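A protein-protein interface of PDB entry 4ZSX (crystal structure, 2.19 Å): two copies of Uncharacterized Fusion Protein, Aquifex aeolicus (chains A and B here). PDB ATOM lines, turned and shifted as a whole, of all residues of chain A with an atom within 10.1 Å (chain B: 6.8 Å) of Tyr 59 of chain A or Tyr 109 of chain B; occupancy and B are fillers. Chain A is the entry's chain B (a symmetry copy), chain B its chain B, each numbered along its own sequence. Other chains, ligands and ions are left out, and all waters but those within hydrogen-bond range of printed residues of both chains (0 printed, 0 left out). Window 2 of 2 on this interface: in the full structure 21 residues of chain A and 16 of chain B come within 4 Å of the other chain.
OG1 of Thr 108 of chain B is in hydrogen-bond range of O of Asp 104 of chain B (2.7 Å).
OH of Tyr 109 of chain B lies within hydrogen-bond range of OD2 of Asp 181 of chain B.
Among the printed residues, pairs that only touch across the chains: Tyr 59 of chain A with Lys 105 of chain B (3.4 Å), Tyr 59 of chain A with Thr 108 of chain B (3.9 Å), Tyr 59 of chain A with Tyr 109 of chain B (3.2 Å), Tyr 59 of chain A with Gln 112 of chain B (3.6 Å) and Trp 60 of chain A with Thr 108 of chain B (3.6 Å).
Tyr 59 of chain A touches just these residues of chain B: Lys 105, Thr 108, Tyr 109 and Gln 112.
Tyr 109 of chain B touches just one residue of chain A: Tyr 59 (3.2 Å).
Of chain A, only Tyr 59 comes within 4 Å of Lys 105 of chain B.
Of the printed residues of chain B, Trp 60 of chain A touches Thr 108.
The nearest residue of chain B that does not touch Tyr 59 of chain A is Glu 106 of chain B (5.7 Å).
The nearest residue of chain A that does not touch Tyr 109 of chain B is Trp 60 of chain A (6.8 Å).
The nearest printed residue of chain B that does not touch Trp 60 of chain A is Gln 112 of chain B (4.9 Å).
Hydrophobic or aromatic side chains of chain A that line the printed part of chain B: Tyr 59 and Trp 60.
Hydrophobic or aromatic side chains of chain B that line the printed part of chain A: Tyr 109.
Among the printed residues, 5 pairs touch across the chains.
Among the printed residues, no Asp or Glu carboxylate lies within 4 Å of a Lys or Arg side-chain nitrogen of the other chain.
No position is printed for both chains.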
ATOM      1  N   PHE A  53      -6.778 -19.702 -33.111  1.00  0.00           N
ATOM      2  CA  PHE A  53      -7.149 -20.983 -32.549  1.00  0.00           C
ATOM      3  C   PHE A  53      -8.648 -20.913 -32.408  1.00  0.00           C
ATOM      4  O   PHE A  53      -9.166 -19.944 -31.885  1.00  0.00           O
ATOM      5  CB  PHE A  53      -6.468 -21.232 -31.207  1.00  0.00           C
ATOM      6  CG  PHE A  53      -6.934 -22.479 -30.502  1.00  0.00           C
ATOM      7  CD1 PHE A  53      -6.676 -23.722 -31.023  1.00  0.00           C
ATOM      8  CD2 PHE A  53      -7.625 -22.400 -29.309  1.00  0.00           C
ATOM      9  CE1 PHE A  53      -7.098 -24.853 -30.371  1.00  0.00           C
ATOM     10  CE2 PHE A  53      -8.043 -23.534 -28.659  1.00  0.00           C
ATOM     11  CZ  PHE A  53      -7.779 -24.759 -29.192  1.00  0.00           C
ATOM     12  N   LEU A  54      -9.344 -21.922 -32.908  1.00  0.00           N
ATOM     13  CA  LEU A  54     -10.796 -21.890 -32.981  1.00  0.00           C
ATOM     14  C   LEU A  54     -11.481 -22.414 -31.748  1.00  0.00           C
ATOM     15  O   LEU A  54     -12.683 -22.232 -31.576  1.00  0.00           O
ATOM     16  CB  LEU A  54     -11.272 -22.707 -34.181  1.00  0.00           C
ATOM     17  CG  LEU A  54     -10.685 -22.304 -35.536  1.00  0.00           C
ATOM     18  CD1 LEU A  54     -11.042 -23.328 -36.580  1.00  0.00           C
ATOM     19  CD2 LEU A  54     -11.191 -20.931 -35.939  1.00  0.00           C
ATOM     20  N   GLY A  55     -10.713 -23.058 -30.885  1.00  0.00           N
ATOM     21  CA  GLY A  55     -11.265 -23.616 -29.671  1.00  0.00           C
ATOM     22  C   GLY A  55     -11.338 -25.122 -29.752  1.00  0.00           C
ATOM     23  O   GLY A  55     -11.260 -25.703 -30.830  1.00  0.00           O
ATOM     24  N   ARG A  56     -11.421 -25.762 -28.596  1.00  0.00           N
ATOM     25  CA  ARG A  56     -11.864 -27.146 -28.534  1.00  0.00           C
ATOM     26  C   ARG A  56     -12.723 -27.373 -27.300  1.00  0.00           C
ATOM     27  O   ARG A  56     -12.189 -27.599 -26.221  1.00  0.00           O
ATOM     28  CB  ARG A  56     -10.696 -28.112 -28.548  1.00  0.00           C
ATOM     29  CG  ARG A  56     -11.175 -29.521 -28.494  1.00  0.00           C
ATOM     30  CD  ARG A  56     -10.052 -30.460 -28.319  1.00  0.00           C
ATOM     31  NE  ARG A  56      -9.268 -30.546 -29.533  1.00  0.00           N
ATOM     32  CZ  ARG A  56      -8.112 -31.183 -29.611  1.00  0.00           C
ATOM     33  NH1 ARG A  56      -7.595 -31.757 -28.541  1.00  0.00           N
ATOM     34  NH2 ARG A  56      -7.463 -31.227 -30.756  1.00  0.00           N
ATOM     35  N   LYS A  57     -14.048 -27.291 -27.466  1.00  0.00           N
ATOM     36  CA  LYS A  57     -14.989 -27.395 -26.355  1.00  0.00           C
ATOM     37  C   LYS A  57     -14.696 -28.658 -25.544  1.00  0.00           C
ATOM     38  O   LYS A  57     -14.328 -29.694 -26.110  1.00  0.00           O
ATOM     39  CB  LYS A  57     -16.455 -27.414 -26.857  1.00  0.00           C
ATOM     40  CG  LYS A  57     -17.147 -26.027 -26.957  1.00  0.00           C
ATOM     41  CD  LYS A  57     -18.502 -25.993 -27.728  1.00  0.00           C
ATOM     42  CE  LYS A  57     -18.375 -26.106 -29.250  1.00  0.00           C
ATOM     43  NZ  LYS A  57     -19.694 -26.052 -29.961  1.00  0.00           N
ATOM     44  N   PRO A  58     -14.831 -28.564 -24.204  1.00  0.00           N
ATOM     45  CA  PRO A  58     -15.228 -27.346 -23.496  1.00  0.00           C
ATOM     46  C   PRO A  58     -14.078 -26.572 -22.862  1.00  0.00           C
ATOM     47  O   PRO A  58     -14.301 -25.447 -22.439  1.00  0.00           O
ATOM     48  CB  PRO A  58     -16.150 -27.880 -22.404  1.00  0.00           C
ATOM     49  CG  PRO A  58     -15.654 -29.273 -22.143  1.00  0.00           C
ATOM     50  CD  PRO A  58     -14.740 -29.698 -23.273  1.00  0.00           C
ATOM     51  N   TYR A  59     -12.877 -27.138 -22.811  1.00  0.00           N
ATOM     52  CA  TYR A  59     -11.838 -26.606 -21.929  1.00  0.00           C
ATOM     53  C   TYR A  59     -10.921 -25.578 -22.584  1.00  0.00           C
ATOM     54  O   TYR A  59     -10.183 -24.888 -21.888  1.00  0.00           O
ATOM     55  CB  TYR A  59     -10.998 -27.756 -21.356  1.00  0.00           C
ATOM     56  CG  TYR A  59     -11.844 -28.810 -20.667  1.00  0.00           C
ATOM     57  CD1 TYR A  59     -12.585 -28.503 -19.532  1.00  0.00           C
ATOM     58  CD2 TYR A  59     -11.933 -30.098 -21.171  1.00  0.00           C
ATOM     59  CE1 TYR A  59     -13.384 -29.449 -18.922  1.00  0.00           C
ATOM     60  CE2 TYR A  59     -12.727 -31.047 -20.557  1.00  0.00           C
ATOM     61  CZ  TYR A  59     -13.445 -30.720 -19.434  1.00  0.00           C
ATOM     62  OH  TYR A  59     -14.233 -31.665 -18.825  1.00  0.00           O
ATOM     63  N   TRP A  60     -10.963 -25.474 -23.909  1.00  0.00           N
ATOM     64  CA  TRP A  60     -10.066 -24.576 -24.635  1.00  0.00           C
ATOM     65  C   TRP A  60     -10.752 -23.490 -25.419  1.00  0.00           C
ATOM     66  O   TRP A  60     -11.390 -23.767 -26.415  1.00  0.00           O
ATOM     67  CB  TRP A  60      -9.216 -25.392 -25.581  1.00  0.00           C
ATOM     68  CG  TRP A  60      -8.395 -26.355 -24.855  1.00  0.00           C
ATOM     69  CD1 TRP A  60      -8.622 -27.681 -24.727  1.00  0.00           C
ATOM     70  CD2 TRP A  60      -7.178 -26.083 -24.173  1.00  0.00           C
ATOM     71  NE1 TRP A  60      -7.628 -28.256 -23.983  1.00  0.00           N
ATOM     72  CE2 TRP A  60      -6.727 -27.291 -23.634  1.00  0.00           C
ATOM     73  CE3 TRP A  60      -6.426 -24.932 -23.966  1.00  0.00           C
ATOM     74  CZ2 TRP A  60      -5.568 -27.383 -22.909  1.00  0.00           C
ATOM     75  CZ3 TRP A  60      -5.282 -25.024 -23.244  1.00  0.00           C
ATOM     76  CH2 TRP A  60      -4.860 -26.242 -22.720  1.00  0.00           C
ATOM     77  N   GLN A  61     -10.599 -22.254 -24.975  1.00  0.00           N
ATOM     78  CA  GLN A  61     -11.206 -21.118 -25.650  1.00  0.00           C
ATOM     79  C   GLN A  61     -10.478 -20.735 -26.926  1.00  0.00           C
ATOM     80  O   GLN A  61      -9.279 -20.952 -27.058  1.00  0.00           O
ATOM     81  CB  GLN A  61     -11.264 -19.904 -24.717  1.00  0.00           C
ATOM     82  CG  GLN A  61     -12.145 -20.076 -23.502  1.00  0.00           C
ATOM     83  CD  GLN A  61     -13.553 -20.527 -23.858  1.00  0.00           C
ATOM     84  OE1 GLN A  61     -14.215 -19.937 -24.720  1.00  0.00           O
ATOM     85  NE2 GLN A  61     -14.013 -21.583 -23.207  1.00  0.00           N
ATOM     86  N   PRO A  62     -11.222 -20.162 -27.876  1.00  0.00           N
ATOM     87  CA  PRO A  62     -10.651 -19.562 -29.070  1.00  0.00           C
ATOM     88  C   PRO A  62      -9.831 -18.354 -28.683  1.00  0.00           C
ATOM     89  O   PRO A  62     -10.091 -17.759 -27.647  1.00  0.00           O
ATOM     90  CB  PRO A  62     -11.880 -19.145 -29.881  1.00  0.00           C
ATOM     91  CG  PRO A  62     -12.998 -19.883 -29.313  1.00  0.00           C
ATOM     92  CD  PRO A  62     -12.688 -20.076 -27.884  1.00  0.00           C
ATOM     93  N   TRP A  63      -8.835 -18.017 -29.481  1.00  0.00           N
ATOM     94  CA  TRP A  63      -8.112 -16.790 -29.279  1.00  0.00           C
ATOM     95  C   TRP A  63      -7.565 -16.409 -30.623  1.00  0.00           C
ATOM     96  O   TRP A  63      -7.529 -17.230 -31.515  1.00  0.00           O
ATOM     97  CB  TRP A  63      -7.021 -16.956 -28.213  1.00  0.00           C
ATOM     98  CG  TRP A  63      -6.082 -18.107 -28.432  1.00  0.00           C
ATOM     99  CD1 TRP A  63      -6.131 -19.324 -27.838  1.00  0.00           C
ATOM    100  CD2 TRP A  63      -4.946 -18.127 -29.297  1.00  0.00           C
ATOM    101  NE1 TRP A  63      -5.105 -20.107 -28.283  1.00  0.00           N
ATOM    102  CE2 TRP A  63      -4.363 -19.394 -29.183  1.00  0.00           C
ATOM    103  CE3 TRP A  63      -4.369 -17.192 -30.165  1.00  0.00           C
ATOM    104  CZ2 TRP A  63      -3.240 -19.755 -29.902  1.00  0.00           C
ATOM    105  CZ3 TRP A  63      -3.264 -17.544 -30.872  1.00  0.00           C
ATOM    106  CH2 TRP A  63      -2.705 -18.818 -30.741  1.00  0.00           C
ATOM    107  N   ARG A  96     -10.610 -13.795 -26.544  1.00  0.00           N
ATOM    108  CA  ARG A  96      -9.268 -13.497 -26.103  1.00  0.00           C
ATOM    109  C   ARG A  96      -8.534 -13.045 -27.309  1.00  0.00           C
ATOM    110  O   ARG A  96      -8.665 -13.649 -28.350  1.00  0.00           O
ATOM    111  CB  ARG A  96      -8.580 -14.711 -25.491  1.00  0.00           C
ATOM    112  CG  ARG A  96      -7.170 -14.403 -24.987  1.00  0.00           C
ATOM    113  CD  ARG A  96      -6.329 -15.642 -24.616  1.00  0.00           C
ATOM    114  NE  ARG A  96      -6.477 -16.080 -23.225  1.00  0.00           N
ATOM    115  CZ  ARG A  96      -5.713 -17.000 -22.633  1.00  0.00           C
ATOM    116  NH1 ARG A  96      -4.706 -17.581 -23.271  1.00  0.00           N
ATOM    117  NH2 ARG A  96      -5.943 -17.329 -21.379  1.00  0.00           N
ATOM    118  N   LYS A 156     -15.735 -13.423 -17.773  1.00  0.00           N
ATOM    119  CA  LYS A 156     -16.548 -14.628 -17.842  1.00  0.00           C
ATOM    120  C   LYS A 156     -17.866 -14.460 -17.098  1.00  0.00           C
ATOM    121  O   LYS A 156     -18.838 -15.116 -17.441  1.00  0.00           O
ATOM    122  CB  LYS A 156     -15.780 -15.850 -17.332  1.00  0.00           C
ATOM    123  CG  LYS A 156     -14.628 -16.260 -18.254  1.00  0.00           C
ATOM    124  CD  LYS A 156     -14.140 -17.688 -18.043  1.00  0.00           C
ATOM    125  CE  LYS A 156     -13.201 -18.083 -19.199  1.00  0.00           C
ATOM    126  NZ  LYS A 156     -13.069 -19.576 -19.418  1.00  0.00           N
ATOM    127  N   ASP B 104      -5.139 -33.708 -24.128  1.00  0.00           N
ATOM    128  CA  ASP B 104      -5.505 -34.558 -23.006  1.00  0.00           C
ATOM    129  C   ASP B 104      -6.622 -33.917 -22.216  1.00  0.00           C
ATOM    130  O   ASP B 104      -6.378 -33.089 -21.363  1.00  0.00           O
ATOM    131  CB  ASP B 104      -4.289 -34.793 -22.118  1.00  0.00           C
ATOM    132  CG  ASP B 104      -4.568 -35.709 -20.952  1.00  0.00           C
ATOM    133  OD1 ASP B 104      -5.732 -36.061 -20.697  1.00  0.00           O
ATOM    134  OD2 ASP B 104      -3.599 -36.114 -20.289  1.00  0.00           O
ATOM    135  N   LYS B 105      -7.850 -34.319 -22.507  1.00  0.00           N
ATOM    136  CA  LYS B 105      -9.047 -33.718 -21.928  1.00  0.00           C
ATOM    137  C   LYS B 105      -9.145 -34.011 -20.454  1.00  0.00           C
ATOM    138  O   LYS B 105      -9.492 -33.159 -19.664  1.00  0.00           O
ATOM    139  CB  LYS B 105     -10.277 -34.264 -22.653  1.00  0.00           C
ATOM    140  CG  LYS B 105     -11.632 -33.903 -22.097  1.00  0.00           C
ATOM    141  CD  LYS B 105     -12.698 -34.798 -22.738  1.00  0.00           C
ATOM    142  CE  LYS B 105     -13.915 -34.015 -23.243  1.00  0.00           C
ATOM    143  NZ  LYS B 105     -14.725 -34.801 -24.234  1.00  0.00           N
ATOM    144  N   GLU B 106      -8.817 -35.231 -20.084  1.00  0.00           N
ATOM    145  CA  GLU B 106      -8.923 -35.613 -18.709  1.00  0.00           C
ATOM    146  C   GLU B 106      -8.026 -34.753 -17.875  1.00  0.00           C
ATOM    147  O   GLU B 106      -8.488 -33.997 -17.046  1.00  0.00           O
ATOM    148  CB  GLU B 106      -8.568 -37.082 -18.528  1.00  0.00           C
ATOM    149  CG  GLU B 106      -8.592 -37.528 -17.072  1.00  0.00           C
ATOM    150  CD  GLU B 106      -8.644 -39.038 -16.903  1.00  0.00           C
ATOM    151  OE1 GLU B 106      -8.697 -39.759 -17.929  1.00  0.00           O
ATOM    152  OE2 GLU B 106      -8.639 -39.499 -15.737  1.00  0.00           O
ATOM    153  N   THR B 107      -6.737 -34.840 -18.144  1.00  0.00           N
ATOM    154  CA  THR B 107      -5.736 -34.125 -17.369  1.00  0.00           C
ATOM    155  C   THR B 107      -5.956 -32.627 -17.364  1.00  0.00           C
ATOM    156  O   THR B 107      -5.857 -31.973 -16.336  1.00  0.00           O
ATOM    157  CB  THR B 107      -4.347 -34.398 -17.913  1.00  0.00           C
ATOM    158  OG1 THR B 107      -4.085 -35.801 -17.872  1.00  0.00           O
ATOM    159  CG2 THR B 107      -3.306 -33.674 -17.113  1.00  0.00           C
ATOM    160  N   THR B 108      -6.241 -32.090 -18.542  1.00  0.00           N
ATOM    161  CA  THR B 108      -6.512 -30.677 -18.713  1.00  0.00           C
ATOM    162  C   THR B 108      -7.582 -30.245 -17.754  1.00  0.00           C
ATOM    163  O   THR B 108      -7.408 -29.313 -16.989  1.00  0.00           O
ATOM    164  CB  THR B 108      -6.972 -30.364 -20.118  1.00  0.00           C
ATOM    165  OG1 THR B 108      -5.863 -30.473 -21.003  1.00  0.00           O
ATOM    166  CG2 THR B 108      -7.501 -28.984 -20.186  1.00  0.00           C
ATOM    167  N   TYR B 109      -8.709 -30.929 -17.816  1.00  0.00           N
ATOM    168  CA  TYR B 109      -9.814 -30.605 -16.950  1.00  0.00           C
ATOM    169  C   TYR B 109      -9.414 -30.609 -15.494  1.00  0.00           C
ATOM    170  O   TYR B 109      -9.758 -29.717 -14.742  1.00  0.00           O
ATOM    171  CB  TYR B 109     -10.947 -31.586 -17.146  1.00  0.00           C
ATOM    172  CG  TYR B 109     -11.919 -31.497 -16.016  1.00  0.00           C
ATOM    173  CD1 TYR B 109     -12.765 -30.405 -15.906  1.00  0.00           C
ATOM    174  CD2 TYR B 109     -11.983 -32.485 -15.044  1.00  0.00           C
ATOM    175  CE1 TYR B 109     -13.657 -30.298 -14.883  1.00  0.00           C
ATOM    176  CE2 TYR B 109     -12.880 -32.388 -14.007  1.00  0.00           C
ATOM    177  CZ  TYR B 109     -13.720 -31.287 -13.934  1.00  0.00           C
ATOM    178  OH  TYR B 109     -14.632 -31.160 -12.912  1.00  0.00           O
ATOM    179  N   GLU B 110      -8.713 -31.652 -15.097  1.00  0.00           N
ATOM    180  CA  GLU B 110      -8.325 -31.808 -13.717  1.00  0.00           C
ATOM    181  C   GLU B 110      -7.413 -30.686 -13.219  1.00  0.00           C
ATOM    182  O   GLU B 110      -7.617 -30.181 -12.127  1.00  0.00           O
ATOM    183  CB  GLU B 110      -7.685 -33.175 -13.538  1.00  0.00           C
ATOM    184  CG  GLU B 110      -8.707 -34.260 -13.812  1.00  0.00           C
ATOM    185  CD  GLU B 110      -8.142 -35.658 -13.783  1.00  0.00           C
ATOM    186  OE1 GLU B 110      -6.934 -35.813 -13.516  1.00  0.00           O
ATOM    187  OE2 GLU B 110      -8.910 -36.602 -14.074  1.00  0.00           O
ATOM    188  N   LEU B 111      -6.422 -30.283 -14.007  1.00  0.00           N
ATOM    189  CA  LEU B 111      -5.506 -29.218 -13.588  1.00  0.00           C
ATOM    190  C   LEU B 111      -6.179 -27.883 -13.409  1.00  0.00           C
ATOM    191  O   LEU B 111      -5.808 -27.088 -12.564  1.00  0.00           O
ATOM    192  CB  LEU B 111      -4.394 -29.024 -14.603  1.00  0.00           C
ATOM    193  CG  LEU B 111      -3.299 -30.055 -14.723  1.00  0.00           C
ATOM    194  CD1 LEU B 111      -2.472 -29.650 -15.892  1.00  0.00           C
ATOM    195  CD2 LEU B 111      -2.477 -30.067 -13.460  1.00  0.00           C
ATOM    196  N   GLN B 112      -7.153 -27.633 -14.257  1.00  0.00           N
ATOM    197  CA  GLN B 112      -7.916 -26.409 -14.221  1.00  0.00           C
ATOM    198  C   GLN B 112      -8.755 -26.337 -12.940  1.00  0.00           C
ATOM    199  O   GLN B 112      -9.197 -25.260 -12.549  1.00  0.00           O
ATOM    200  CB  GLN B 112      -8.775 -26.307 -15.484  1.00  0.00           C
ATOM    201  CG  GLN B 112      -7.924 -26.079 -16.735  1.00  0.00           C
ATOM    202  CD  GLN B 112      -8.729 -25.804 -17.991  1.00  0.00           C
ATOM    203  OE1 GLN B 112      -9.949 -25.965 -18.010  1.00  0.00           O
ATOM    204  NE2 GLN B 112      -8.045 -25.385 -19.053  1.00  0.00           N
ATOM    205  N   LYS B 113      -8.982 -27.487 -12.307  1.00  0.00           N
ATOM    206  CA  LYS B 113      -9.662 -27.551 -11.013  1.00  0.00           C
ATOM    207  C   LYS B 113      -8.712 -27.592  -9.841  1.00  0.00           C
ATOM    208  O   LYS B 113      -9.130 -27.810  -8.728  1.00  0.00           O
ATOM    209  CB  LYS B 113     -10.602 -28.754 -10.946  1.00  0.00           C
ATOM    210  CG  LYS B 113     -11.946 -28.489 -11.578  1.00  0.00           C
ATOM    211  CD  LYS B 113     -12.541 -27.248 -10.912  1.00  0.00           C
ATOM    212  CE  LYS B 113     -13.920 -26.868 -11.395  1.00  0.00           C
ATOM    213  NZ  LYS B 113     -14.177 -25.460 -10.995  1.00  0.00           N
ATOM    214  N   GLY B 114      -7.429 -27.395 -10.083  1.00  0.00           N
ATOM    215  CA  GLY B 114      -6.506 -27.209  -8.986  1.00  0.00           C
ATOM    216  C   GLY B 114      -5.817 -28.433  -8.430  1.00  0.00           C
ATOM    217  O   GLY B 114      -5.063 -28.317  -7.475  1.00  0.00           O
ATOM    218  N   VAL B 115      -6.020 -29.592  -9.040  1.00  0.00           N
ATOM    219  CA  VAL B 115      -5.336 -30.802  -8.606  1.00  0.00           C
ATOM    220  C   VAL B 115      -3.842 -30.555  -8.644  1.00  0.00           C
ATOM    221  O   VAL B 115      -3.361 -29.976  -9.605  1.00  0.00           O
ATOM    222  CB  VAL B 115      -5.673 -31.968  -9.516  1.00  0.00           C
ATOM    223  CG1 VAL B 115      -4.892 -33.184  -9.121  1.00  0.00           C
ATOM    224  CG2 VAL B 115      -7.128 -32.239  -9.460  1.00  0.00           C
ATOM    225  N   ASP B 181     -15.908 -31.388  -5.658  1.00  0.00           N
ATOM    226  CA  ASP B 181     -16.367 -32.345  -6.669  1.00  0.00           C
ATOM    227  C   ASP B 181     -16.190 -33.773  -6.142  1.00  0.00           C
ATOM    228  O   ASP B 181     -15.062 -34.243  -6.000  1.00  0.00           O
ATOM    229  CB  ASP B 181     -15.600 -32.163  -7.986  1.00  0.00           C
ATOM    230  CG  ASP B 181     -16.152 -33.025  -9.134  1.00  0.00           C
ATOM    231  OD1 ASP B 181     -16.839 -34.042  -8.888  1.00  0.00           O
ATOM    232  OD2 ASP B 181     -15.874 -32.690 -10.307  1.00  0.00           O
ATOM    233  N   LEU B 184     -14.217 -36.053  -8.518  1.00  0.00           N
ATOM    234  CA  LEU B 184     -12.829 -35.670  -8.648  1.00  0.00           C
ATOM    235  C   LEU B 184     -12.029 -36.057  -7.417  1.00  0.00           C
ATOM    236  O   LEU B 184     -10.942 -36.617  -7.534  1.00  0.00           O
ATOM    237  CB  LEU B 184     -12.708 -34.172  -8.920  1.00  0.00           C
ATOM    238  CG  LEU B 184     -11.289 -33.667  -9.205  1.00  0.00           C
ATOM    239  CD1 LEU B 184     -10.633 -34.560 -10.222  1.00  0.00           C
ATOM    240  CD2 LEU B 184     -11.266 -32.221  -9.688  1.00  0.00           C
ATOM    241  N   LYS B 187     -11.148 -39.744  -7.229  1.00  0.00           N
ATOM    242  CA  LYS B 187     -10.086 -40.079  -8.154  1.00  0.00           C
ATOM    243  C   LYS B 187      -8.751 -39.673  -7.570  1.00  0.00           C
ATOM    244  O   LYS B 187      -7.814 -40.456  -7.546  1.00  0.00           O
ATOM    245  CB  LYS B 187     -10.310 -39.415  -9.507  1.00  0.00           C
ATOM    246  CG  LYS B 187      -9.865 -40.267 -10.678  1.00  0.00           C
ATOM    247  CD  LYS B 187     -10.299 -39.649 -11.985  1.00  0.00           C
ATOM    248  CE  LYS B 187     -11.739 -39.192 -11.909  1.00  0.00           C
ATOM    249  NZ  LYS B 187     -12.181 -38.610 -13.205  1.00  0.00           N
